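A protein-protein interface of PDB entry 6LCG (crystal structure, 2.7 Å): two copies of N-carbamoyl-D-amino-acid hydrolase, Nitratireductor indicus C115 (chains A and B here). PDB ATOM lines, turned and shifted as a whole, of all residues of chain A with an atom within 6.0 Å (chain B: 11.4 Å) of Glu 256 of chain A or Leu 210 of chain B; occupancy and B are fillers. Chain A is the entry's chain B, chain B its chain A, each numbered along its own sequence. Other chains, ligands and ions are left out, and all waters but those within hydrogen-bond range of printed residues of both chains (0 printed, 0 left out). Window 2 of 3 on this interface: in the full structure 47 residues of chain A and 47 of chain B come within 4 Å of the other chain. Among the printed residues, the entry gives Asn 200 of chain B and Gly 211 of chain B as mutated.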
ATOM      1  N   GLN A 220       2.893  -7.639  20.094  1.00  0.00           N
ATOM      2  CA  GLN A 220       2.284  -8.682  19.276  1.00  0.00           C
ATOM      3  C   GLN A 220       2.365  -8.348  17.793  1.00  0.00           C
ATOM      4  O   GLN A 220       2.461  -9.256  16.958  1.00  0.00           O
ATOM      5  CB  GLN A 220       0.830  -8.899  19.693  1.00  0.00           C
ATOM      6  CG  GLN A 220       0.665  -9.449  21.100  1.00  0.00           C
ATOM      7  CD  GLN A 220      -0.786  -9.682  21.470  1.00  0.00           C
ATOM      8  OE1 GLN A 220      -1.363  -8.937  22.263  1.00  0.00           O
ATOM      9  NE2 GLN A 220      -1.383 -10.720  20.897  1.00  0.00           N
ATOM     10  N   ILE A 250       5.737 -13.194  26.698  1.00  0.00           N
ATOM     11  CA  ILE A 250       6.585 -13.804  25.682  1.00  0.00           C
ATOM     12  C   ILE A 250       5.705 -14.066  24.469  1.00  0.00           C
ATOM     13  O   ILE A 250       4.680 -14.753  24.579  1.00  0.00           O
ATOM     14  CB  ILE A 250       7.244 -15.100  26.181  1.00  0.00           C
ATOM     15  CG1 ILE A 250       8.214 -14.799  27.326  1.00  0.00           C
ATOM     16  CG2 ILE A 250       7.966 -15.806  25.041  1.00  0.00           C
ATOM     17  CD1 ILE A 250       8.897 -16.026  27.887  1.00  0.00           C
ATOM     18  N   VAL A 251       6.089 -13.512  23.323  1.00  0.00           N
ATOM     19  CA  VAL A 251       5.248 -13.505  22.133  1.00  0.00           C
ATOM     20  C   VAL A 251       5.887 -14.367  21.054  1.00  0.00           C
ATOM     21  O   VAL A 251       7.093 -14.272  20.798  1.00  0.00           O
ATOM     22  CB  VAL A 251       5.012 -12.072  21.618  1.00  0.00           C
ATOM     23  CG1 VAL A 251       3.965 -12.071  20.515  1.00  0.00           C
ATOM     24  CG2 VAL A 251       4.591 -11.162  22.760  1.00  0.00           C
ATOM     25  N   ALA A 252       5.069 -15.199  20.417  1.00  0.00           N
ATOM     26  CA  ALA A 252       5.498 -16.049  19.321  1.00  0.00           C
ATOM     27  C   ALA A 252       5.569 -15.254  18.020  1.00  0.00           C
ATOM     28  O   ALA A 252       5.000 -14.163  17.919  1.00  0.00           O
ATOM     29  CB  ALA A 252       4.535 -17.225  19.173  1.00  0.00           C
ATOM     30  N   PRO A 253       6.272 -15.772  17.006  1.00  0.00           N
ATOM     31  CA  PRO A 253       6.298 -15.087  15.702  1.00  0.00           C
ATOM     32  C   PRO A 253       4.929 -14.932  15.060  1.00  0.00           C
ATOM     33  O   PRO A 253       4.806 -14.170  14.092  1.00  0.00           O
ATOM     34  CB  PRO A 253       7.208 -15.983  14.850  1.00  0.00           C
ATOM     35  CG  PRO A 253       8.068 -16.685  15.837  1.00  0.00           C
ATOM     36  CD  PRO A 253       7.203 -16.914  17.041  1.00  0.00           C
ATOM     37  N   THR A 254       3.909 -15.631  15.551  1.00  0.00           N
ATOM     38  CA  THR A 254       2.544 -15.448  15.081  1.00  0.00           C
ATOM     39  C   THR A 254       1.839 -14.281  15.758  1.00  0.00           C
ATOM     40  O   THR A 254       0.677 -14.010  15.437  1.00  0.00           O
ATOM     41  CB  THR A 254       1.731 -16.725  15.305  1.00  0.00           C
ATOM     42  OG1 THR A 254       1.756 -17.068  16.698  1.00  0.00           O
ATOM     43  CG2 THR A 254       2.306 -17.874  14.493  1.00  0.00           C
ATOM     44  N   GLY A 255       2.508 -13.587  16.677  1.00  0.00           N
ATOM     45  CA  GLY A 255       1.877 -12.547  17.457  1.00  0.00           C
ATOM     46  C   GLY A 255       1.097 -13.035  18.656  1.00  0.00           C
ATOM     47  O   GLY A 255       0.490 -12.214  19.355  1.00  0.00           O
ATOM     48  N   GLU A 256       1.094 -14.339  18.920  1.00  0.00           N
ATOM     49  CA  GLU A 256       0.350 -14.887  20.043  1.00  0.00           C
ATOM     50  C   GLU A 256       1.169 -14.809  21.324  1.00  0.00           C
ATOM     51  O   GLU A 256       2.389 -14.989  21.312  1.00  0.00           O
ATOM     52  CB  GLU A 256      -0.039 -16.340  19.765  1.00  0.00           C
ATOM     53  CG  GLU A 256      -1.064 -16.510  18.658  1.00  0.00           C
ATOM     54  CD  GLU A 256      -1.380 -17.965  18.382  1.00  0.00           C
ATOM     55  OE1 GLU A 256      -0.430 -18.762  18.225  1.00  0.00           O
ATOM     56  OE2 GLU A 256      -2.578 -18.315  18.330  1.00  0.00           O
ATOM     57  N   ILE A 257       0.486 -14.540  22.432  1.00  0.00           N
ATOM     58  CA  ILE A 257       1.115 -14.516  23.747  1.00  0.00           C
ATOM     59  C   ILE A 257       1.110 -15.934  24.303  1.00  0.00           C
ATOM     60  O   ILE A 257       0.045 -16.506  24.559  1.00  0.00           O
ATOM     61  CB  ILE A 257       0.391 -13.547  24.693  1.00  0.00           C
ATOM     62  CG1 ILE A 257       0.532 -12.108  24.194  1.00  0.00           C
ATOM     63  CG2 ILE A 257       0.927 -13.684  26.110  1.00  0.00           C
ATOM     64  CD1 ILE A 257      -0.135 -11.084  25.083  1.00  0.00           C
ATOM     65  N   VAL A 258       2.302 -16.507  24.483  1.00  0.00           N
ATOM     66  CA  VAL A 258       2.425 -17.861  25.017  1.00  0.00           C
ATOM     67  C   VAL A 258       2.726 -17.879  26.509  1.00  0.00           C
ATOM     68  O   VAL A 258       2.606 -18.942  27.140  1.00  0.00           O
ATOM     69  CB  VAL A 258       3.500 -18.668  24.256  1.00  0.00           C
ATOM     70  CG1 VAL A 258       3.103 -18.830  22.797  1.00  0.00           C
ATOM     71  CG2 VAL A 258       4.855 -17.993  24.373  1.00  0.00           C
ATOM     72  N   ARG A 277      10.225 -21.733  13.993  1.00  0.00           N
ATOM     73  CA  ARG A 277       8.883 -21.246  13.692  1.00  0.00           C
ATOM     74  C   ARG A 277       8.912 -19.901  12.980  1.00  0.00           C
ATOM     75  O   ARG A 277       7.925 -19.531  12.335  1.00  0.00           O
ATOM     76  CB  ARG A 277       8.057 -21.142  14.974  1.00  0.00           C
ATOM     77  CG  ARG A 277       7.750 -22.477  15.632  1.00  0.00           C
ATOM     78  CD  ARG A 277       6.920 -22.281  16.888  1.00  0.00           C
ATOM     79  NE  ARG A 277       5.686 -21.552  16.614  1.00  0.00           N
ATOM     80  CZ  ARG A 277       4.837 -21.139  17.549  1.00  0.00           C
ATOM     81  NH1 ARG A 277       5.088 -21.380  18.829  1.00  0.00           N
ATOM     82  NH2 ARG A 277       3.738 -20.483  17.205  1.00  0.00           N
ATOM     83  N   TYR A 281       6.879 -17.900   8.167  1.00  0.00           N
ATOM     84  CA  TYR A 281       6.394 -16.686   7.523  1.00  0.00           C
ATOM     85  C   TYR A 281       7.462 -15.960   6.717  1.00  0.00           C
ATOM     86  O   TYR A 281       7.116 -15.217   5.791  1.00  0.00           O
ATOM     87  CB  TYR A 281       5.814 -15.728   8.569  1.00  0.00           C
ATOM     88  CG  TYR A 281       4.508 -16.197   9.173  1.00  0.00           C
ATOM     89  CD1 TYR A 281       3.790 -17.239   8.598  1.00  0.00           C
ATOM     90  CD2 TYR A 281       3.988 -15.593  10.310  1.00  0.00           C
ATOM     91  CE1 TYR A 281       2.595 -17.669   9.142  1.00  0.00           C
ATOM     92  CE2 TYR A 281       2.793 -16.016  10.862  1.00  0.00           C
ATOM     93  CZ  TYR A 281       2.101 -17.054  10.273  1.00  0.00           C
ATOM     94  OH  TYR A 281       0.911 -17.479  10.819  1.00  0.00           O
ATOM     95  N   ARG B 174      -1.885  -3.476   4.246  1.00  0.00           N
ATOM     96  CA  ARG B 174      -2.127  -3.332   5.677  1.00  0.00           C
ATOM     97  C   ARG B 174      -1.234  -4.227   6.527  1.00  0.00           C
ATOM     98  O   ARG B 174      -1.160  -4.018   7.742  1.00  0.00           O
ATOM     99  CB  ARG B 174      -3.598  -3.627   5.984  1.00  0.00           C
ATOM    100  CG  ARG B 174      -3.978  -5.102   5.926  1.00  0.00           C
ATOM    101  CD  ARG B 174      -5.485  -5.270   5.801  1.00  0.00           C
ATOM    102  NE  ARG B 174      -5.929  -6.640   6.041  1.00  0.00           N
ATOM    103  CZ  ARG B 174      -6.014  -7.576   5.102  1.00  0.00           C
ATOM    104  NH1 ARG B 174      -5.679  -7.294   3.851  1.00  0.00           N
ATOM    105  NH2 ARG B 174      -6.432  -8.796   5.413  1.00  0.00           N
ATOM    106  N   ARG B 175      -0.566  -5.208   5.927  1.00  0.00           N
ATOM    107  CA  ARG B 175       0.338  -6.096   6.646  1.00  0.00           C
ATOM    108  C   ARG B 175       1.750  -5.539   6.766  1.00  0.00           C
ATOM    109  O   ARG B 175       2.590  -6.158   7.426  1.00  0.00           O
ATOM    110  CB  ARG B 175       0.378  -7.464   5.960  1.00  0.00           C
ATOM    111  CG  ARG B 175      -0.830  -8.337   6.253  1.00  0.00           C
ATOM    112  CD  ARG B 175      -1.112  -9.292   5.109  1.00  0.00           C
ATOM    113  NE  ARG B 175       0.108  -9.902   4.592  1.00  0.00           N
ATOM    114  CZ  ARG B 175       0.142 -10.758   3.575  1.00  0.00           C
ATOM    115  NH1 ARG B 175      -0.981 -11.109   2.963  1.00  0.00           N
ATOM    116  NH2 ARG B 175       1.299 -11.261   3.169  1.00  0.00           N
ATOM    117  N   TYR B 195      -9.965  -4.796   1.153  1.00  0.00           N
ATOM    118  CA  TYR B 195      -9.124  -5.977   1.037  1.00  0.00           C
ATOM    119  C   TYR B 195      -9.936  -7.195   0.625  1.00  0.00           C
ATOM    120  O   TYR B 195     -11.114  -7.325   0.966  1.00  0.00           O
ATOM    121  CB  TYR B 195      -8.375  -6.262   2.346  1.00  0.00           C
ATOM    122  CG  TYR B 195      -9.241  -6.623   3.531  1.00  0.00           C
ATOM    123  CD1 TYR B 195      -9.779  -5.639   4.348  1.00  0.00           C
ATOM    124  CD2 TYR B 195      -9.489  -7.951   3.854  1.00  0.00           C
ATOM    125  CE1 TYR B 195     -10.559  -5.966   5.442  1.00  0.00           C
ATOM    126  CE2 TYR B 195     -10.265  -8.287   4.945  1.00  0.00           C
ATOM    127  CZ  TYR B 195     -10.797  -7.291   5.736  1.00  0.00           C
ATOM    128  OH  TYR B 195     -11.573  -7.624   6.822  1.00  0.00           O
ATOM    129  N   THR B 197      -9.070 -11.042   1.169  1.00  0.00           N
ATOM    130  CA  THR B 197      -8.149 -11.997   1.773  1.00  0.00           C
ATOM    131  C   THR B 197      -8.739 -13.397   1.702  1.00  0.00           C
ATOM    132  O   THR B 197      -9.733 -13.679   2.388  1.00  0.00           O
ATOM    133  CB  THR B 197      -7.853 -11.615   3.224  1.00  0.00           C
ATOM    134  OG1 THR B 197      -7.283 -10.301   3.264  1.00  0.00           O
ATOM    135  CG2 THR B 197      -6.875 -12.600   3.842  1.00  0.00           C
ATOM    136  N   PRO B 198      -8.182 -14.294   0.892  1.00  0.00           N
ATOM    137  CA  PRO B 198      -8.720 -15.656   0.817  1.00  0.00           C
ATOM    138  C   PRO B 198      -8.476 -16.428   2.104  1.00  0.00           C
ATOM    139  O   PRO B 198      -7.638 -16.072   2.935  1.00  0.00           O
ATOM    140  CB  PRO B 198      -7.954 -16.283  -0.356  1.00  0.00           C
ATOM    141  CG  PRO B 198      -7.396 -15.123  -1.123  1.00  0.00           C
ATOM    142  CD  PRO B 198      -7.120 -14.066  -0.101  1.00  0.00           C
ATOM    143  N   VAL B 199      -9.236 -17.509   2.257  1.00  0.00           N
ATOM    144  CA  VAL B 199      -9.128 -18.402   3.403  1.00  0.00           C
ATOM    145  C   VAL B 199      -8.932 -19.819   2.885  1.00  0.00           C
ATOM    146  O   VAL B 199      -9.730 -20.304   2.076  1.00  0.00           O
ATOM    147  CB  VAL B 199     -10.369 -18.323   4.312  1.00  0.00           C
ATOM    148  CG1 VAL B 199     -10.278 -19.352   5.428  1.00  0.00           C
ATOM    149  CG2 VAL B 199     -10.518 -16.921   4.885  1.00  0.00           C
ATOM    150  N   ASN B 200      -7.870 -20.476   3.344  1.00  0.00           N
ATOM    151  CA  ASN B 200      -7.608 -21.852   2.943  1.00  0.00           C
ATOM    152  C   ASN B 200      -8.626 -22.787   3.582  1.00  0.00           C
ATOM    153  O   ASN B 200      -8.901 -22.697   4.783  1.00  0.00           O
ATOM    154  CB  ASN B 200      -6.190 -22.261   3.337  1.00  0.00           C
ATOM    155  CG  ASN B 200      -5.135 -21.646   2.437  1.00  0.00           C
ATOM    156  OD1 ASN B 200      -5.294 -21.603   1.216  1.00  0.00           O
ATOM    157  ND2 ASN B 200      -4.051 -21.166   3.036  1.00  0.00           N
ATOM    158  N   SER B 202     -10.104 -25.564   5.503  1.00  0.00           N
ATOM    159  CA  SER B 202      -9.620 -26.393   6.607  1.00  0.00           C
ATOM    160  C   SER B 202      -8.134 -26.164   6.876  1.00  0.00           C
ATOM    161  O   SER B 202      -7.309 -27.048   6.649  1.00  0.00           O
ATOM    162  CB  SER B 202      -9.881 -27.876   6.322  1.00  0.00           C
ATOM    163  OG  SER B 202      -9.459 -28.684   7.407  1.00  0.00           O
ATOM    164  N   SER B 207      -5.360 -21.771  11.190  1.00  0.00           N
ATOM    165  CA  SER B 207      -6.805 -21.811  11.374  1.00  0.00           C
ATOM    166  C   SER B 207      -7.451 -20.516  10.896  1.00  0.00           C
ATOM    167  O   SER B 207      -6.782 -19.649  10.332  1.00  0.00           O
ATOM    168  CB  SER B 207      -7.154 -22.060  12.843  1.00  0.00           C
ATOM    169  OG  SER B 207      -6.747 -20.972  13.655  1.00  0.00           O
ATOM    170  N   GLU B 208      -8.758 -20.390  11.124  1.00  0.00           N
ATOM    171  CA  GLU B 208      -9.475 -19.169  10.778  1.00  0.00           C
ATOM    172  C   GLU B 208      -9.421 -18.127  11.884  1.00  0.00           C
ATOM    173  O   GLU B 208      -9.420 -16.924  11.592  1.00  0.00           O
ATOM    174  CB  GLU B 208     -10.937 -19.481  10.446  1.00  0.00           C
ATOM    175  CG  GLU B 208     -11.130 -20.325   9.198  1.00  0.00           C
ATOM    176  CD  GLU B 208     -12.583 -20.409   8.773  1.00  0.00           C
ATOM    177  OE1 GLU B 208     -13.410 -19.655   9.329  1.00  0.00           O
ATOM    178  OE2 GLU B 208     -12.899 -21.226   7.883  1.00  0.00           O
ATOM    179  N   THR B 209      -9.381 -18.558  13.148  1.00  0.00           N
ATOM    180  CA  THR B 209      -9.245 -17.608  14.247  1.00  0.00           C
ATOM    181  C   THR B 209      -7.910 -16.878  14.188  1.00  0.00           C
ATOM    182  O   THR B 209      -7.815 -15.721  14.614  1.00  0.00           O
ATOM    183  CB  THR B 209      -9.397 -18.326  15.589  1.00  0.00           C
ATOM    184  OG1 THR B 209      -8.400 -19.350  15.701  1.00  0.00           O
ATOM    185  CG2 THR B 209     -10.778 -18.954  15.703  1.00  0.00           C
ATOM    186  N   LEU B 210      -6.873 -17.533  13.662  1.00  0.00           N
ATOM    187  CA  LEU B 210      -5.575 -16.883  13.519  1.00  0.00           C
ATOM    188  C   LEU B 210      -5.563 -15.919  12.340  1.00  0.00           C
ATOM    189  O   LEU B 210      -4.921 -14.865  12.403  1.00  0.00           O
ATOM    190  CB  LEU B 210      -4.477 -17.936  13.360  1.00  0.00           C
ATOM    191  CG  LEU B 210      -3.054 -17.493  13.709  1.00  0.00           C
ATOM    192  CD1 LEU B 210      -2.923 -17.257  15.206  1.00  0.00           C
ATOM    193  CD2 LEU B 210      -2.032 -18.513  13.232  1.00  0.00           C
ATOM    194  N   GLY B 211      -6.265 -16.263  11.257  1.00  0.00           N
ATOM    195  CA  GLY B 211      -6.331 -15.366  10.115  1.00  0.00           C
ATOM    196  C   GLY B 211      -7.083 -14.086  10.423  1.00  0.00           C
ATOM    197  O   GLY B 211      -6.681 -13.001   9.995  1.00  0.00           O
ATOM    198  N   MET B 212      -8.187 -14.194  11.168  1.00  0.00           N
ATOM    199  CA  MET B 212      -8.902 -13.000  11.604  1.00  0.00           C
ATOM    200  C   MET B 212      -8.099 -12.220  12.635  1.00  0.00           C
ATOM    201  O   MET B 212      -8.175 -10.986  12.676  1.00  0.00           O
ATOM    202  CB  MET B 212     -10.266 -13.387  12.175  1.00  0.00           C
ATOM    203  CG  MET B 212     -11.157 -12.204  12.509  1.00  0.00           C
ATOM    204  SD  MET B 212     -11.589 -11.248  11.045  1.00  0.00           S
ATOM    205  CE  MET B 212     -12.515 -12.466  10.115  1.00  0.00           C
ATOM    206  N   PHE B 213      -7.326 -12.918  13.472  1.00  0.00           N
ATOM    207  CA  PHE B 213      -6.483 -12.240  14.450  1.00  0.00           C
ATOM    208  C   PHE B 213      -5.409 -11.404  13.766  1.00  0.00           C
ATOM    209  O   PHE B 213      -5.162 -10.258  14.156  1.00  0.00           O
ATOM    210  CB  PHE B 213      -5.854 -13.266  15.395  1.00  0.00           C
ATOM    211  CG  PHE B 213      -4.748 -12.712  16.248  1.00  0.00           C
ATOM    212  CD1 PHE B 213      -5.030 -11.877  17.316  1.00  0.00           C
ATOM    213  CD2 PHE B 213      -3.427 -13.039  15.991  1.00  0.00           C
ATOM    214  CE1 PHE B 213      -4.015 -11.370  18.105  1.00  0.00           C
ATOM    215  CE2 PHE B 213      -2.408 -12.537  16.776  1.00  0.00           C
ATOM    216  CZ  PHE B 213      -2.702 -11.702  17.835  1.00  0.00           C
ATOM    217  N   HIS B 214      -4.761 -11.959  12.738  1.00  0.00           N
ATOM    218  CA  HIS B 214      -3.737 -11.209  12.021  1.00  0.00           C
ATOM    219  C   HIS B 214      -4.336 -10.060  11.221  1.00  0.00           C
ATOM    220  O   HIS B 214      -3.672  -9.035  11.020  1.00  0.00           O
ATOM    221  CB  HIS B 214      -2.950 -12.140  11.099  1.00  0.00           C
ATOM    222  CG  HIS B 214      -2.103 -13.137  11.828  1.00  0.00           C
ATOM    223  ND1 HIS B 214      -1.757 -14.355  11.286  1.00  0.00           N
ATOM    224  CD2 HIS B 214      -1.528 -13.092  13.052  1.00  0.00           C
ATOM    225  CE1 HIS B 214      -1.009 -15.020  12.148  1.00  0.00           C
ATOM    226  NE2 HIS B 214      -0.855 -14.276  13.228  1.00  0.00           N
ATOM    227  N   ASN B 215      -5.579 -10.208  10.758  1.00  0.00           N
ATOM    228  CA  ASN B 215      -6.215  -9.141   9.993  1.00  0.00           C
ATOM    229  C   ASN B 215      -6.423  -7.897  10.848  1.00  0.00           C
ATOM    230  O   ASN B 215      -6.144  -6.777  10.403  1.00  0.00           O
ATOM    231  CB  ASN B 215      -7.547  -9.630   9.422  1.00  0.00           C
ATOM    232  CG  ASN B 215      -8.266  -8.561   8.621  1.00  0.00           C
ATOM    233  OD1 ASN B 215      -7.636  -7.709   7.993  1.00  0.00           O
ATOM    234  ND2 ASN B 215      -9.593  -8.600   8.643  1.00  0.00           N
ATOM    235  N   HIS B 216      -6.900  -8.074  12.081  1.00  0.00           N
ATOM    236  CA  HIS B 216      -7.156  -6.934  12.952  1.00  0.00           C
ATOM    237  C   HIS B 216      -5.897  -6.459  13.666  1.00  0.00           C
ATOM    238  O   HIS B 216      -5.769  -5.263  13.947  1.00  0.00           O
ATOM    239  CB  HIS B 216      -8.233  -7.289  13.977  1.00  0.00           C
ATOM    240  CG  HIS B 216      -9.555  -7.631  13.365  1.00  0.00           C
ATOM    241  ND1 HIS B 216     -10.533  -8.326  14.045  1.00  0.00           N
ATOM    242  CD2 HIS B 216     -10.064  -7.372  12.138  1.00  0.00           C
ATOM    243  CE1 HIS B 216     -11.584  -8.482  13.261  1.00  0.00           C
ATOM    244  NE2 HIS B 216     -11.326  -7.911  12.098  1.00  0.00           N
ATOM    245  N   LEU B 217      -4.966  -7.369  13.965  1.00  0.00           N
ATOM    246  CA  LEU B 217      -3.749  -6.980  14.672  1.00  0.00           C
ATOM    247  C   LEU B 217      -2.952  -5.950  13.882  1.00  0.00           C
ATOM    248  O   LEU B 217      -2.432  -4.986  14.456  1.00  0.00           O
ATOM    249  CB  LEU B 217      -2.893  -8.212  14.961  1.00  0.00           C
ATOM    250  CG  LEU B 217      -1.544  -7.969  15.638  1.00  0.00           C
ATOM    251  CD1 LEU B 217      -1.734  -7.357  17.015  1.00  0.00           C
ATOM    252  CD2 LEU B 217      -0.752  -9.263  15.726  1.00  0.00           C
ATOM    253  N   THR B 218      -2.844  -6.134  12.565  1.00  0.00           N
ATOM    254  CA  THR B 218      -2.069  -5.200  11.756  1.00  0.00           C
ATOM    255  C   THR B 218      -2.757  -3.845  11.652  1.00  0.00           C
ATOM    256  O   THR B 218      -2.082  -2.811  11.591  1.00  0.00           O
ATOM    257  CB  THR B 218      -1.831  -5.777  10.361  1.00  0.00           C
ATOM    258  OG1 THR B 218      -3.088  -6.015   9.716  1.00  0.00           O
ATOM    259  CG2 THR B 218      -1.056  -7.083  10.451  1.00  0.00           C
ATOM    260  N   MET B 219      -4.091  -3.829  11.633  1.00  0.00           N
ATOM    261  CA  MET B 219      -4.818  -2.569  11.536  1.00  0.00           C
ATOM    262  C   MET B 219      -4.877  -1.848  12.877  1.00  0.00           C
ATOM    263  O   MET B 219      -4.681  -0.630  12.937  1.00  0.00           O
ATOM    264  CB  MET B 219      -6.226  -2.817  11.000  1.00  0.00           C
ATOM    265  CG  MET B 219      -6.268  -3.119   9.519  1.00  0.00           C
ATOM    266  SD  MET B 219      -7.931  -3.468   8.932  1.00  0.00           S
ATOM    267  CE  MET B 219      -7.752  -3.036   7.207  1.00  0.00           C
ATOM    268  N   GLN B 220      -5.153  -2.580  13.959  1.00  0.00           N
ATOM    269  CA  GLN B 220      -5.178  -1.963  15.279  1.00  0.00           C
ATOM    270  C   GLN B 220      -3.814  -1.409  15.663  1.00  0.00           C
ATOM    271  O   GLN B 220      -3.730  -0.406  16.381  1.00  0.00           O
ATOM    272  CB  GLN B 220      -5.655  -2.971  16.324  1.00  0.00           C
ATOM    273  CG  GLN B 220      -7.090  -3.421  16.135  1.00  0.00           C
ATOM    274  CD  GLN B 220      -7.510  -4.458  17.152  1.00  0.00           C
ATOM    275  OE1 GLN B 220      -7.636  -5.641  16.834  1.00  0.00           O
ATOM    276  NE2 GLN B 220      -7.730  -4.021  18.387  1.00  0.00           N
ATOM    277  N   MET B 245     -12.204 -13.829   3.442  1.00  0.00           N
ATOM    278  CA  MET B 245     -12.297 -13.404   4.831  1.00  0.00           C
ATOM    279  C   MET B 245     -13.194 -12.179   4.963  1.00  0.00           C
ATOM    280  O   MET B 245     -13.205 -11.299   4.097  1.00  0.00           O
ATOM    281  CB  MET B 245     -10.905 -13.097   5.382  1.00  0.00           C
ATOM    282  CG  MET B 245     -10.883 -12.679   6.843  1.00  0.00           C
ATOM    283  SD  MET B 245      -9.251 -12.143   7.390  1.00  0.00           S
ATOM    284  CE  MET B 245      -8.294 -13.629   7.106  1.00  0.00           C
ATOM    285  N   GLY B 246     -13.953 -12.132   6.053  1.00  0.00           N
ATOM    286  CA  GLY B 246     -14.774 -10.978   6.356  1.00  0.00           C
ATOM    287  C   GLY B 246     -14.159 -10.106   7.429  1.00  0.00           C
ATOM    288  O   GLY B 246     -13.008  -9.674   7.304  1.00  0.00           O
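Printed residues of chain B within 4 Å of Glu 256 of chain A: Leu 210. Leu 210 of chain B touches two residues of chain A. Gln 220 of chain A touches two residues of chain B. No residue of chain B comes within 4 Å of Val 251 of chain A. Of the printed residues of chain B, Thr 254 of chain A touches Phe 213 (3.7 Å) and His 214 (2.7 Å). Of chain B, only Phe 213 comes within 4 Å of Gly 255 of chain A. No residue of chain B comes within 4 Å of Ile 257 of chain A. Printed residues of chain A within 4 Å of His 214 of chain B: Thr 254 (2.7 Å) and Tyr 281 (3.4 Å). Printed residues of chain A within 4 Å of Leu 217 of chain B: Gln 220 (3.4 Å). Printed residues of chain B within 4 Å of Tyr 281 of chain A: Leu 210 (3.9 Å) and His 214 (3.4 Å). Of the printed residues of chain A, Phe 213 of chain B touches Gln 220, Thr 254 and Gly 255. Arg 174 of chain B touches none of the printed residues of chain A. The nearest residue of chain B that does not touch Glu 256 of chain A is Phe 213 of chain B (4.5 Å). The nearest residue of chain A that does not touch Leu 210 of chain B is Thr 254 of chain A (4.6 Å). The nearest printed residue of chain B that does not touch Tyr 281 of chain A is Gly 211 of chain B (7.3 Å).
The side-chain hydroxyl of Ser 207 of chain B sits at hydrogen-bond distance from the backbone NH of Leu 210 of chain B (3.4 Å). The backbone carbonyl oxygen (O) of Leu 210 of chain B lies close to a ring nitrogen (ND1) of His 214 of chain B (3.4 Å). O of His 214 of chain B lies close to OG1 of Thr 218 of chain B (3.3 Å). O of Gly 255 of chain A sits at hydrogen-bond distance from NE2 of Gln 220 of chain A (2.8 Å). The side-chain hydroxyl of Thr 254 of chain A sits at hydrogen-bond distance from the side-chain carboxylate of Glu 256 of chain A (3.2 Å).
NE2 of His 214 of chain B is in hydrogen-bond range of O of Thr 254 of chain A, at 2.7 Å.
1 position is printed for both chains.
Printed residues of chain B that touch a printed residue of chain A: Leu 210, Phe 213, His 214 and Leu 217. Hydrophobic or aromatic side chains of chain A within 4 Å of the printed part of chain B: Tyr 281. Among the printed residues, no Asp or Glu carboxylate lies within 4 Å of a Lys or Arg side-chain nitrogen of the other chain.
Among the printed residues, pairs that only touch across the chains: Glu 256 of chain A with Leu 210 of chain B (3.3 Å), Tyr 281 of chain A with His 214 of chain B (3.4 Å), Gln 220 of chain A with Leu 217 of chain B (3.4 Å), Gln 220 of chain A with Phe 213 of chain B (3.5 Å), Gly 255 of chain A with Phe 213 of chain B (3.6 Å), Thr 254 of chain A with Phe 213 of chain B (3.7 Å) and Tyr 281 of chain A with Leu 210 of chain B (3.9 Å).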
